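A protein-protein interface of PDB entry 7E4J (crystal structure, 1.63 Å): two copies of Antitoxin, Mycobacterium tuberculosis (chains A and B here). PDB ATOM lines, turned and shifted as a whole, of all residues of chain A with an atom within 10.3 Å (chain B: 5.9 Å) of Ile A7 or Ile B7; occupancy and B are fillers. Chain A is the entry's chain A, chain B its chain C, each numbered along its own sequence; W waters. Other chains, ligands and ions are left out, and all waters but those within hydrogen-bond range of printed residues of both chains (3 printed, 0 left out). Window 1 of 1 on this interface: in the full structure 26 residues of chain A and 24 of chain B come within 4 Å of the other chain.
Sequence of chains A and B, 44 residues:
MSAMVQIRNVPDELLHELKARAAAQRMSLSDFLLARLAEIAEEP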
ATOM      1  N   SER A   2      -7.168  -2.147   9.603  1.00  0.00           N
ATOM      2  CA  SER A   2      -8.113  -3.255   9.896  1.00  0.00           C
ATOM      3  C   SER A   2      -9.446  -3.014   9.187  1.00  0.00           C
ATOM      4  O   SER A   2      -9.688  -1.863   8.698  1.00  0.00           O
ATOM      5  CB  SER A   2      -8.330  -3.417  11.394  1.00  0.00           C
ATOM      6  OG  SER A   2      -9.086  -2.334  11.933  1.00  0.00           O
ATOM      7  N   ALA A   3     -10.284  -4.046   9.151  1.00  0.00           N
ATOM      8  CA  ALA A   3     -11.623  -4.008   8.509  1.00  0.00           C
ATOM      9  C   ALA A   3     -12.585  -4.950   9.227  1.00  0.00           C
ATOM     10  O   ALA A   3     -12.118  -5.987   9.772  1.00  0.00           O
ATOM     11  CB  ALA A   3     -11.528  -4.395   7.054  1.00  0.00           C
ATOM     12  N   MET A   4     -13.856  -4.551   9.242  1.00  0.00           N
ATOM     13  CA  MET A   4     -14.986  -5.376   9.729  1.00  0.00           C
ATOM     14  C   MET A   4     -15.271  -6.464   8.699  1.00  0.00           C
ATOM     15  O   MET A   4     -15.330  -6.150   7.498  1.00  0.00           O
ATOM     16  CB  MET A   4     -16.252  -4.541   9.909  1.00  0.00           C
ATOM     17  CG  MET A   4     -17.442  -5.359  10.361  1.00  0.00           C
ATOM     18  SD  MET A   4     -18.783  -4.296  10.970  1.00  0.00           S
ATOM     19  CE  MET A   4     -17.975  -2.703  11.162  1.00  0.00           C
ATOM     20  N   VAL A   5     -15.424  -7.718   9.157  1.00  0.00           N
ATOM     21  CA  VAL A   5     -15.628  -8.902   8.278  1.00  0.00           C
ATOM     22  C   VAL A   5     -17.013  -9.446   8.613  1.00  0.00           C
ATOM     23  O   VAL A   5     -17.351  -9.503   9.799  1.00  0.00           O
ATOM     24  CB  VAL A   5     -14.526  -9.966   8.439  1.00  0.00           C
ATOM     25  CG1 VAL A   5     -14.896 -11.257   7.728  1.00  0.00           C
ATOM     26  CG2 VAL A   5     -13.180  -9.468   7.946  1.00  0.00           C
ATOM     27  N   GLN A   6     -17.808  -9.723   7.572  1.00  0.00           N
ATOM     28  CA  GLN A   6     -19.207 -10.192   7.676  1.00  0.00           C
ATOM     29  C   GLN A   6     -19.268 -11.612   7.132  1.00  0.00           C
ATOM     30  O   GLN A   6     -18.785 -11.848   6.005  1.00  0.00           O
ATOM     31  CB  GLN A   6     -20.106  -9.243   6.883  1.00  0.00           C
ATOM     32  CG  GLN A   6     -20.409  -7.954   7.644  1.00  0.00           C
ATOM     33  CD  GLN A   6     -20.381  -6.708   6.788  1.00  0.00           C
ATOM     34  OE1 GLN A   6     -21.307  -5.897   6.815  1.00  0.00           O
ATOM     35  NE2 GLN A   6     -19.326  -6.560   6.004  1.00  0.00           N
ATOM     36  N   ILE A   7     -19.820 -12.517   7.934  1.00  0.00           N
ATOM     37  CA  ILE A   7     -20.029 -13.949   7.590  1.00  0.00           C
ATOM     38  C   ILE A   7     -21.537 -14.130   7.405  1.00  0.00           C
ATOM     39  O   ILE A   7     -22.278 -13.852   8.363  1.00  0.00           O
ATOM     40  CB  ILE A   7     -19.432 -14.846   8.685  1.00  0.00           C
ATOM     41  CG1 ILE A   7     -17.958 -14.503   8.937  1.00  0.00           C
ATOM     42  CG2 ILE A   7     -19.621 -16.322   8.366  1.00  0.00           C
ATOM     43  CD1 ILE A   7     -17.377 -15.133  10.177  1.00  0.00           C
ATOM     44  N   ARG A   8     -21.935 -14.477   6.177  1.00  0.00           N
ATOM     45  CA  ARG A   8     -23.335 -14.618   5.716  1.00  0.00           C
ATOM     46  C   ARG A   8     -23.813 -16.037   6.015  1.00  0.00           C
ATOM     47  O   ARG A   8     -22.950 -16.944   6.171  1.00  0.00           O
ATOM     48  CB  ARG A   8     -23.422 -14.319   4.212  1.00  0.00           C
ATOM     49  CG  ARG A   8     -23.190 -12.856   3.868  1.00  0.00           C
ATOM     50  CD  ARG A   8     -23.489 -12.563   2.401  1.00  0.00           C
ATOM     51  NE  ARG A   8     -22.307 -12.743   1.562  1.00  0.00           N
ATOM     52  CZ  ARG A   8     -22.201 -12.388   0.273  1.00  0.00           C
ATOM     53  NH1 ARG A   8     -23.223 -11.850  -0.376  1.00  0.00           N
ATOM     54  NH2 ARG A   8     -21.067 -12.598  -0.376  1.00  0.00           N
ATOM     55  N   ASN A   9     -25.135 -16.202   6.081  1.00  0.00           N
ATOM     56  CA  ASN A   9     -25.841 -17.508   6.153  1.00  0.00           C
ATOM     57  C   ASN A   9     -25.341 -18.294   7.364  1.00  0.00           C
ATOM     58  O   ASN A   9     -25.084 -19.510   7.211  1.00  0.00           O
ATOM     59  CB  ASN A   9     -25.653 -18.303   4.857  1.00  0.00           C
ATOM     60  CG  ASN A   9     -25.940 -17.466   3.631  1.00  0.00           C
ATOM     61  OD1 ASN A   9     -25.165 -17.468   2.675  1.00  0.00           O
ATOM     62  ND2 ASN A   9     -27.032 -16.719   3.667  1.00  0.00           N
ATOM     63  N   VAL A  10     -25.160 -17.630   8.508  1.00  0.00           N
ATOM     64  CA  VAL A  10     -24.905 -18.343   9.787  1.00  0.00           C
ATOM     65  C   VAL A  10     -26.255 -18.847  10.298  1.00  0.00           C
ATOM     66  O   VAL A  10     -27.133 -18.058  10.659  1.00  0.00           O
ATOM     67  CB  VAL A  10     -24.187 -17.482  10.831  1.00  0.00           C
ATOM     68  CG1 VAL A  10     -23.892 -18.309  12.066  1.00  0.00           C
ATOM     69  CG2 VAL A  10     -22.921 -16.861  10.255  1.00  0.00           C
ATOM     70  N   PRO A  11     -26.468 -20.176  10.383  1.00  0.00           N
ATOM     71  CA  PRO A  11     -27.720 -20.715  10.934  1.00  0.00           C
ATOM     72  C   PRO A  11     -27.956 -20.321  12.407  1.00  0.00           C
ATOM     73  O   PRO A  11     -27.000 -20.168  13.175  1.00  0.00           O
ATOM     74  CB  PRO A  11     -27.548 -22.235  10.781  1.00  0.00           C
ATOM     75  CG  PRO A  11     -26.514 -22.361   9.676  1.00  0.00           C
ATOM     76  CD  PRO A  11     -25.537 -21.234   9.971  1.00  0.00           C
ATOM     77  N   LEU A  14     -26.255 -22.426  15.171  1.00  0.00           N
ATOM     78  CA  LEU A  14     -24.804 -22.180  15.200  1.00  0.00           C
ATOM     79  C   LEU A  14     -24.537 -20.831  15.885  1.00  0.00           C
ATOM     80  O   LEU A  14     -23.622 -20.798  16.731  1.00  0.00           O
ATOM     81  CB  LEU A  14     -24.250 -22.226  13.776  1.00  0.00           C
ATOM     82  CG  LEU A  14     -22.761 -21.911  13.620  1.00  0.00           C
ATOM     83  CD1 LEU A  14     -21.912 -22.719  14.580  1.00  0.00           C
ATOM     84  CD2 LEU A  14     -22.325 -22.144  12.182  1.00  0.00           C
ATOM     85  N   LEU A  15     -25.272 -19.778  15.522  1.00  0.00           N
ATOM     86  CA  LEU A  15     -24.985 -18.438  16.096  1.00  0.00           C
ATOM     87  C   LEU A  15     -25.159 -18.456  17.622  1.00  0.00           C
ATOM     88  O   LEU A  15     -24.313 -17.908  18.358  1.00  0.00           O
ATOM     89  CB  LEU A  15     -25.880 -17.383  15.449  1.00  0.00           C
ATOM     90  CG  LEU A  15     -25.437 -15.947  15.727  1.00  0.00           C
ATOM     91  CD1 LEU A  15     -23.927 -15.799  15.681  1.00  0.00           C
ATOM     92  CD2 LEU A  15     -26.061 -14.978  14.740  1.00  0.00           C
ATOM     93  N   LEU A  18     -22.208 -20.213  19.306  1.00  0.00           N
ATOM     94  CA  LEU A  18     -21.013 -19.331  19.344  1.00  0.00           C
ATOM     95  C   LEU A  18     -21.185 -18.255  20.440  1.00  0.00           C
ATOM     96  O   LEU A  18     -20.160 -17.931  21.126  1.00  0.00           O
ATOM     97  CB  LEU A  18     -20.811 -18.701  17.970  1.00  0.00           C
ATOM     98  CG  LEU A  18     -20.508 -19.655  16.813  1.00  0.00           C
ATOM     99  CD1 LEU A  18     -20.556 -18.891  15.506  1.00  0.00           C
ATOM    100  CD2 LEU A  18     -19.181 -20.375  16.995  1.00  0.00           C
ATOM    101  N   SER A  28     -17.241 -10.508  24.149  1.00  0.00           N
ATOM    102  CA  SER A  28     -18.161 -10.243  23.022  1.00  0.00           C
ATOM    103  C   SER A  28     -17.987 -11.357  21.971  1.00  0.00           C
ATOM    104  O   SER A  28     -16.881 -11.960  21.921  1.00  0.00           O
ATOM    105  CB  SER A  28     -17.922  -8.886  22.455  1.00  0.00           C
ATOM    106  OG  SER A  28     -16.768  -8.830  21.646  1.00  0.00           O
ATOM    107  N   LEU A  29     -19.058 -11.697  21.220  1.00  0.00           N
ATOM    108  CA  LEU A  29     -18.958 -12.620  20.060  1.00  0.00           C
ATOM    109  C   LEU A  29     -17.799 -12.200  19.135  1.00  0.00           C
ATOM    110  O   LEU A  29     -17.005 -13.090  18.734  1.00  0.00           O
ATOM    111  CB  LEU A  29     -20.288 -12.685  19.306  1.00  0.00           C
ATOM    112  CG  LEU A  29     -20.317 -13.622  18.098  1.00  0.00           C
ATOM    113  CD1 LEU A  29     -20.050 -15.063  18.492  1.00  0.00           C
ATOM    114  CD2 LEU A  29     -21.629 -13.521  17.366  1.00  0.00           C
ATOM    115  N   SER A  30     -17.709 -10.907  18.786  1.00  0.00           N
ATOM    116  CA  SER A  30     -16.659 -10.359  17.877  1.00  0.00           C
ATOM    117  C   SER A  30     -15.263 -10.637  18.456  1.00  0.00           C
ATOM    118  O   SER A  30     -14.440 -11.188  17.725  1.00  0.00           O
ATOM    119  CB  SER A  30     -16.856  -8.900  17.610  1.00  0.00           C
ATOM    120  OG  SER A  30     -15.832  -8.428  16.759  1.00  0.00           O
ATOM    121  N   ASP A  31     -15.037 -10.339  19.746  1.00  0.00           N
ATOM    122  CA  ASP A  31     -13.704 -10.542  20.394  1.00  0.00           C
ATOM    123  C   ASP A  31     -13.361 -12.038  20.392  1.00  0.00           C
ATOM    124  O   ASP A  31     -12.222 -12.408  20.015  1.00  0.00           O
ATOM    125  CB  ASP A  31     -13.673 -10.027  21.835  1.00  0.00           C
ATOM    126  CG  ASP A  31     -13.475  -8.537  22.023  1.00  0.00           C
ATOM    127  OD1 ASP A  31     -13.616  -7.790  21.055  1.00  0.00           O
ATOM    128  OD2 ASP A  31     -13.217  -8.164  23.174  1.00  0.00           O
ATOM    129  N   PHE A  32     -14.357 -12.882  20.699  1.00  0.00           N
ATOM    130  CA  PHE A  32     -14.179 -14.347  20.788  1.00  0.00           C
ATOM    131  C   PHE A  32     -13.749 -14.865  19.404  1.00  0.00           C
ATOM    132  O   PHE A  32     -12.778 -15.628  19.282  1.00  0.00           O
ATOM    133  CB  PHE A  32     -15.473 -15.003  21.244  1.00  0.00           C
ATOM    134  CG  PHE A  32     -15.449 -16.500  21.114  1.00  0.00           C
ATOM    135  CD1 PHE A  32     -14.679 -17.290  21.955  1.00  0.00           C
ATOM    136  CD2 PHE A  32     -16.205 -17.120  20.134  1.00  0.00           C
ATOM    137  CE1 PHE A  32     -14.679 -18.670  21.819  1.00  0.00           C
ATOM    138  CE2 PHE A  32     -16.234 -18.502  20.034  1.00  0.00           C
ATOM    139  CZ  PHE A  32     -15.452 -19.281  20.858  1.00  0.00           C
ATOM    140  N   LEU A  33     -14.472 -14.447  18.374  1.00  0.00           N
ATOM    141  CA  LEU A  33     -14.259 -14.937  16.993  1.00  0.00           C
ATOM    142  C   LEU A  33     -12.910 -14.416  16.482  1.00  0.00           C
ATOM    143  O   LEU A  33     -12.125 -15.232  15.880  1.00  0.00           O
ATOM    144  CB  LEU A  33     -15.442 -14.548  16.108  1.00  0.00           C
ATOM    145  CG  LEU A  33     -16.713 -15.362  16.363  1.00  0.00           C
ATOM    146  CD1 LEU A  33     -17.762 -15.059  15.312  1.00  0.00           C
ATOM    147  CD2 LEU A  33     -16.429 -16.857  16.368  1.00  0.00           C
ATOM    148  N   LEU A  34     -12.616 -13.158  16.779  1.00  0.00           N
ATOM    149  CA  LEU A  34     -11.322 -12.574  16.344  1.00  0.00           C
ATOM    150  C   LEU A  34     -10.191 -13.414  16.946  1.00  0.00           C
ATOM    151  O   LEU A  34      -9.275 -13.799  16.198  1.00  0.00           O
ATOM    152  CB  LEU A  34     -11.251 -11.104  16.759  1.00  0.00           C
ATOM    153  CG  LEU A  34     -10.024 -10.366  16.230  1.00  0.00           C
ATOM    154  CD1 LEU A  34      -9.814 -10.614  14.734  1.00  0.00           C
ATOM    155  CD2 LEU A  34     -10.133  -8.876  16.490  1.00  0.00           C
ATOM    156  N   ALA A  35     -10.273 -13.743  18.233  1.00  0.00           N
ATOM    157  CA  ALA A  35      -9.204 -14.483  18.948  1.00  0.00           C
ATOM    158  C   ALA A  35      -9.045 -15.884  18.367  1.00  0.00           C
ATOM    159  O   ALA A  35      -7.884 -16.302  18.194  1.00  0.00           O
ATOM    160  CB  ALA A  35      -9.480 -14.553  20.415  1.00  0.00           C
ATOM    161  N   ARG A  36     -10.144 -16.568  18.029  1.00  0.00           N
ATOM    162  CA  ARG A  36     -10.083 -17.962  17.505  1.00  0.00           C
ATOM    163  C   ARG A  36      -9.492 -17.950  16.090  1.00  0.00           C
ATOM    164  O   ARG A  36      -8.640 -18.829  15.787  1.00  0.00           O
ATOM    165  CB  ARG A  36     -11.462 -18.624  17.469  1.00  0.00           C
ATOM    166  CG  ARG A  36     -12.038 -18.971  18.836  1.00  0.00           C
ATOM    167  CD  ARG A  36     -11.108 -19.715  19.794  1.00  0.00           C
ATOM    168  NE  ARG A  36     -10.794 -21.075  19.377  1.00  0.00           N
ATOM    169  CZ  ARG A  36     -11.412 -22.184  19.808  1.00  0.00           C
ATOM    170  NH1 ARG A  36     -12.382 -22.134  20.715  1.00  0.00           N
ATOM    171  NH2 ARG A  36     -11.042 -23.365  19.328  1.00  0.00           N
ATOM    172  N   LEU A  37      -9.921 -16.988  15.261  1.00  0.00           N
ATOM    173  CA  LEU A  37      -9.391 -16.862  13.888  1.00  0.00           C
ATOM    174  C   LEU A  37      -7.895 -16.562  13.956  1.00  0.00           C
ATOM    175  O   LEU A  37      -7.161 -17.101  13.139  1.00  0.00           O
ATOM    176  CB  LEU A  37     -10.183 -15.798  13.138  1.00  0.00           C
ATOM    177  CG  LEU A  37     -11.613 -16.252  12.853  1.00  0.00           C
ATOM    178  CD1 LEU A  37     -12.387 -15.142  12.171  1.00  0.00           C
ATOM    179  CD2 LEU A  37     -11.615 -17.532  12.033  1.00  0.00           C
ATOM    180  N   ALA A  38      -7.443 -15.782  14.929  1.00  0.00           N
ATOM    181  CA  ALA A  38      -6.010 -15.443  15.063  1.00  0.00           C
ATOM    182  C   ALA A  38      -5.219 -16.703  15.437  1.00  0.00           C
ATOM    183  O   ALA A  38      -4.110 -16.900  14.889  1.00  0.00           O
ATOM    184  CB  ALA A  38      -5.813 -14.340  16.074  1.00  0.00           C
ATOM    185  N   ILE A  40      -6.154 -19.854  14.703  1.00  0.00           N
ATOM    186  CA  ILE A  40      -6.201 -20.680  13.456  1.00  0.00           C
ATOM    187  C   ILE A  40      -5.069 -20.244  12.516  1.00  0.00           C
ATOM    188  O   ILE A  40      -4.310 -21.109  12.056  1.00  0.00           O
ATOM    189  CB  ILE A  40      -7.584 -20.585  12.772  1.00  0.00           C
ATOM    190  CG1 ILE A  40      -8.654 -21.345  13.561  1.00  0.00           C
ATOM    191  CG2 ILE A  40      -7.516 -21.059  11.327  1.00  0.00           C
ATOM    192  CD1 ILE A  40     -10.074 -20.941  13.228  1.00  0.00           C
ATOM    193  N   ALA B   3     -28.461 -15.772   9.944  1.00  0.00           N
ATOM    194  CA  ALA B   3     -28.053 -14.508  10.596  1.00  0.00           C
ATOM    195  C   ALA B   3     -26.706 -14.026  10.059  1.00  0.00           C
ATOM    196  O   ALA B   3     -25.877 -14.863   9.679  1.00  0.00           O
ATOM    197  CB  ALA B   3     -27.978 -14.691  12.089  1.00  0.00           C
ATOM    198  N   MET B   4     -26.546 -12.705  10.013  1.00  0.00           N
ATOM    199  CA  MET B   4     -25.252 -12.022   9.783  1.00  0.00           C
ATOM    200  C   MET B   4     -24.434 -12.110  11.075  1.00  0.00           C
ATOM    201  O   MET B   4     -25.013 -11.864  12.150  1.00  0.00           O
ATOM    202  CB  MET B   4     -25.491 -10.548   9.419  1.00  0.00           C
ATOM    203  CG  MET B   4     -24.233  -9.724   9.197  1.00  0.00           C
ATOM    204  SD  MET B   4     -23.336 -10.248   7.738  1.00  0.00           S
ATOM    205  CE  MET B   4     -24.530  -9.879   6.451  1.00  0.00           C
ATOM    206  N   VAL B   5     -23.139 -12.398  10.965  1.00  0.00           N
ATOM    207  CA  VAL B   5     -22.142 -12.177  12.053  1.00  0.00           C
ATOM    208  C   VAL B   5     -21.205 -11.058  11.579  1.00  0.00           C
ATOM    209  O   VAL B   5     -20.805 -11.080  10.389  1.00  0.00           O
ATOM    210  CB  VAL B   5     -21.391 -13.479  12.409  1.00  0.00           C
ATOM    211  CG1 VAL B   5     -20.083 -13.238  13.176  1.00  0.00           C
ATOM    212  CG2 VAL B   5     -22.294 -14.457  13.148  1.00  0.00           C
ATOM    213  N   GLN B   6     -20.887 -10.108  12.465  1.00  0.00           N
ATOM    214  CA  GLN B   6     -19.887  -9.040  12.212  1.00  0.00           C
ATOM    215  C   GLN B   6     -18.697  -9.269  13.133  1.00  0.00           C
ATOM    216  O   GLN B   6     -18.915  -9.322  14.356  1.00  0.00           O
ATOM    217  CB  GLN B   6     -20.524  -7.673  12.387  1.00  0.00           C
ATOM    218  CG  GLN B   6     -21.493  -7.312  11.277  1.00  0.00           C
ATOM    219  CD  GLN B   6     -21.586  -5.818  11.112  1.00  0.00           C
ATOM    220  OE1 GLN B   6     -21.745  -5.078  12.077  1.00  0.00           O
ATOM    221  NE2 GLN B   6     -21.438  -5.356   9.885  1.00  0.00           N
ATOM    222  N   ILE B   7     -17.505  -9.342  12.560  1.00  0.00           N
ATOM    223  CA  ILE B   7     -16.220  -9.350  13.319  1.00  0.00           C
ATOM    224  C   ILE B   7     -15.536  -8.010  13.026  1.00  0.00           C
ATOM    225  O   ILE B   7     -15.228  -7.787  11.840  1.00  0.00           O
ATOM    226  CB  ILE B   7     -15.321 -10.541  12.951  1.00  0.00           C
ATOM    227  CG1 ILE B   7     -16.087 -11.865  12.936  1.00  0.00           C
ATOM    228  CG2 ILE B   7     -14.133 -10.586  13.898  1.00  0.00           C
ATOM    229  CD1 ILE B   7     -15.241 -13.038  12.496  1.00  0.00           C
ATOM    230  N   ARG B   8     -15.413  -7.159  14.052  1.00  0.00           N
ATOM    231  CA  ARG B   8     -14.837  -5.791  13.945  1.00  0.00           C
ATOM    232  C   ARG B   8     -13.312  -5.896  14.060  1.00  0.00           C
ATOM    233  O   ARG B   8     -12.830  -6.843  14.702  1.00  0.00           O
ATOM    234  CB  ARG B   8     -15.427  -4.857  15.007  1.00  0.00           C
ATOM    235  CG  ARG B   8     -16.935  -4.679  14.912  1.00  0.00           C
ATOM    236  CD  ARG B   8     -17.547  -3.729  15.918  1.00  0.00           C
ATOM    237  NE  ARG B   8     -17.742  -4.320  17.233  1.00  0.00           N
ATOM    238  CZ  ARG B   8     -18.572  -5.336  17.527  1.00  0.00           C
ATOM    239  NH1 ARG B   8     -19.294  -5.935  16.586  1.00  0.00           N
ATOM    240  NH2 ARG B   8     -18.653  -5.768  18.776  1.00  0.00           N
ATOM    241  N   ASN B   9     -12.607  -5.013  13.359  1.00  0.00           N
ATOM    242  CA  ASN B   9     -11.170  -4.710  13.544  1.00  0.00           C
ATOM    243  C   ASN B   9     -10.345  -5.973  13.352  1.00  0.00           C
ATOM    244  O   ASN B   9      -9.471  -6.257  14.207  1.00  0.00           O
ATOM    245  CB  ASN B   9     -10.940  -4.080  14.911  1.00  0.00           C
ATOM    246  CG  ASN B   9     -11.856  -2.896  15.118  1.00  0.00           C
ATOM    247  OD1 ASN B   9     -12.043  -2.102  14.209  1.00  0.00           O
ATOM    248  ND2 ASN B   9     -12.433  -2.765  16.310  1.00  0.00           N
ATOM    249  N   VAL B  10     -10.613  -6.691  12.267  1.00  0.00           N
ATOM    250  CA  VAL B  10      -9.694  -7.747  11.768  1.00  0.00           C
ATOM    251  C   VAL B  10      -8.479  -7.056  11.131  1.00  0.00           C
ATOM    252  O   VAL B  10      -8.596  -6.370  10.109  1.00  0.00           O
ATOM    253  CB  VAL B  10     -10.377  -8.709  10.784  1.00  0.00           C
ATOM    254  CG1 VAL B  10      -9.399  -9.814  10.387  1.00  0.00           C
ATOM    255  CG2 VAL B  10     -11.708  -9.203  11.320  1.00  0.00           C
ATOM    256  N   SER B  30     -16.244 -15.931   3.189  1.00  0.00           N
ATOM    257  CA  SER B  30     -17.466 -16.177   4.000  1.00  0.00           C
ATOM    258  C   SER B  30     -17.674 -17.684   4.191  1.00  0.00           C
ATOM    259  O   SER B  30     -17.858 -18.104   5.322  1.00  0.00           O
ATOM    260  CB  SER B  30     -18.669 -15.519   3.402  1.00  0.00           C
ATOM    261  OG  SER B  30     -19.810 -15.783   4.207  1.00  0.00           O
ATOM    262  N   LEU B  33     -14.895 -19.122   6.429  1.00  0.00           N
ATOM    263  CA  LEU B  33     -15.105 -18.677   7.842  1.00  0.00           C
ATOM    264  C   LEU B  33     -16.336 -19.392   8.422  1.00  0.00           C
ATOM    265  O   LEU B  33     -16.320 -19.763   9.570  1.00  0.00           O
ATOM    266  CB  LEU B  33     -15.230 -17.154   7.899  1.00  0.00           C
ATOM    267  CG  LEU B  33     -13.939 -16.374   7.616  1.00  0.00           C
ATOM    268  CD1 LEU B  33     -14.143 -14.906   7.893  1.00  0.00           C
ATOM    269  CD2 LEU B  33     -12.714 -16.892   8.374  1.00  0.00           C
ATOM    270  N   LEU B  34     -17.382 -19.603   7.649  1.00  0.00           N
ATOM    271  CA  LEU B  34     -18.558 -20.386   8.124  1.00  0.00           C
ATOM    272  C   LEU B  34     -18.073 -21.790   8.532  1.00  0.00           C
ATOM    273  O   LEU B  34     -18.422 -22.242   9.610  1.00  0.00           O
ATOM    274  CB  LEU B  34     -19.602 -20.407   7.009  1.00  0.00           C
ATOM    275  CG  LEU B  34     -20.871 -21.201   7.282  1.00  0.00           C
ATOM    276  CD1 LEU B  34     -21.500 -20.793   8.612  1.00  0.00           C
ATOM    277  CD2 LEU B  34     -21.850 -21.004   6.136  1.00  0.00           C
ATOM    278  N   LEU B  37     -16.090 -21.453  11.898  1.00  0.00           N
ATOM    279  CA  LEU B  37     -17.058 -21.148  12.971  1.00  0.00           C
ATOM    280  C   LEU B  37     -17.765 -22.451  13.373  1.00  0.00           C
ATOM    281  O   LEU B  37     -17.942 -22.676  14.572  1.00  0.00           O
ATOM    282  CB  LEU B  37     -18.052 -20.085  12.483  1.00  0.00           C
ATOM    283  CG  LEU B  37     -17.823 -18.639  12.946  1.00  0.00           C
ATOM    284  CD1 LEU B  37     -16.361 -18.219  12.839  1.00  0.00           C
ATOM    285  CD2 LEU B  37     -18.717 -17.693  12.158  1.00  0.00           C
HETATM  286  O   HOH W   1     -26.829 -14.350   6.389  1.00  0.00           O
HETATM  287  O   HOH W   2     -13.562  -7.788  17.851  1.00  0.00           O
HETATM  288  O   HOH W   3     -20.215  -5.104  14.381  1.00  0.00           O
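Water W1 bridges the backbone NH (N) of Asn A9 (2.5 Å) and the backbone carbonyl oxygen (O) of Ala B3 (3.5 Å).
Water W3 lies within hydrogen-bond range of NH1 of Arg B8 (2.5 Å), OE1 of Gln B6 (2.8 Å) and SD of Met A4 (3.8 Å).
Water W2 lies within hydrogen-bond range of the side-chain hydroxyl of Ser A30 (2.6 Å), the side-chain carboxylate of Asp A31 (3.2 Å) and the backbone carbonyl oxygen of Arg B8 (3.4 Å).
The backbone NH (N) of Val B10 lies within hydrogen-bond range of the backbone carbonyl oxygen (O) of Ala A3 (3.0 Å).
NE2 of Gln B6 lies within hydrogen-bond range of SD of Met A4 (3.1 Å).
The backbone NH (N) of Val A5 is in hydrogen-bond range of the backbone carbonyl oxygen (O) of Ile B7, at 2.7 Å.
OE1 of Gln A6 lies within hydrogen-bond range of NE2 of Gln B6 (3.1 Å).
The backbone NH of Ile A7 lies within hydrogen-bond range of the backbone carbonyl oxygen of Val B5, at 3.0 Å.
OG of Ser B30 lies within hydrogen-bond range of N of Arg A8.
O of Val A10 sits at hydrogen-bond distance from N of Ala B3, 2.7 Å away.
The side-chain hydroxyl (OG) of Ser A30 is in hydrogen-bond range of the backbone NH (N) of Arg B8.
Of the 25 printed residues of chain A, 16 touch a printed residue of chain B.
Hydrophobic or aromatic side chains of chain A that line the printed part of chain B: Met A4, Val A5, Ile A7, Val A10, Leu A14, Leu A15, Leu A18, Leu A33, Leu A34 and Leu A37.
Printed residues of chain B that touch a printed residue of chain A: Ala B3, Met B4, Val B5, Gln B6, Ile B7, Arg B8, Asn B9, Val B10, Ser B30, Leu B33, Leu B34 and Leu B37.
Among the printed residues, 41 pairs touch across the chains.
Among the printed residues, no Asp or Glu carboxylate lies within 4 Å of a Lys or Arg side-chain nitrogen of the other chain.
Met A4 touches Ile B7, and with the chains exchanged Ile A7 touches Met B4.
Ile A7 touches Leu B37, and with the chains exchanged Leu A37 touches Ile B7.
Asn A9 touches Leu B34, and with the chains exchanged Leu A34 touches Asn B9.
Leu A33 touches Leu B37, and with the chains exchanged Leu A37 touches Leu B33.
Positions printed for both chains: 3, 4, 5, 6, 7, 8, 9, 10, 30, 33, 34 and 37.
Of the 41 pairs that touch across the chains among the printed residues, 31 have their exchanged pair printed and touching as well.
CA of Asn B9 touches OG of Ser A2, 3.5 Å away.
Ala A3 touches Asn B9 (O to N, 3.7 Å).
Val A5 touches Val B5 (O to O, 3.8 Å).
Ile B7 touches Ile A7 (CD1 to CD1, 3.8 Å).
CD2 of Leu B37 touches CD1 of Ile A7, 3.5 Å away.
Leu A15 touches Val B5 (CD1 to CG2, 3.3 Å).
Ser A30 touches Gln B6.
Ser A30 touches Ile B7.
CB of Leu A33 touches CD1 of Ile B7, 3.9 Å away.
CD2 of Leu A34 touches O of Asn B9, 3.5 Å away.
Ile A7 touches just these residues of chain B: Ala B3 (3.96 Å), Met B4 (3.8 Å), Val B5 (3.0 Å), Ile B7 (3.8 Å), Ser B30 (3.9 Å), Leu B33 (3.7 Å) and Leu B37 (3.5 Å).
Printed residues of chain B within 4 Å of Leu A14: Leu B34 (3.9 Å) and Leu B37 (3.97 Å).
Leu A29 touches none of the printed residues of chain B.
Arg A36 touches none of the printed residues of chain B.
Printed residues of chain B within 4 Å of Leu A37: Ile B7 (3.6 Å) and Leu B33 (3.9 Å).
Of chain A, only Gln A6 and Ile A7 come within 4 Å of Met B4.
Ile B7 touches just these residues of chain A: Met A4, Val A5, Ile A7, Ser A30, Leu A33 and Leu A37.
Printed residues of chain A within 4 Å of Asn B9: Ser A2 (3.5 Å), Ala A3 (3.7 Å) and Leu A34 (3.5 Å).
Of the printed residues of chain A, Val B10 touches Ser A2, Ala A3 and Val A5.
Of chain A, only Val A5 (3.7 Å), Ile A7 (3.7 Å) and Leu A37 (3.9 Å) come within 4 Å of Leu B33.
Leu B34 touches two residues of chain A.
The nearest residue of chain B that does not touch Ile A7 is Leu B34 (4.04 Å).
The nearest residue of chain A that does not touch Ile B7 is Leu A34 (4.1 Å).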
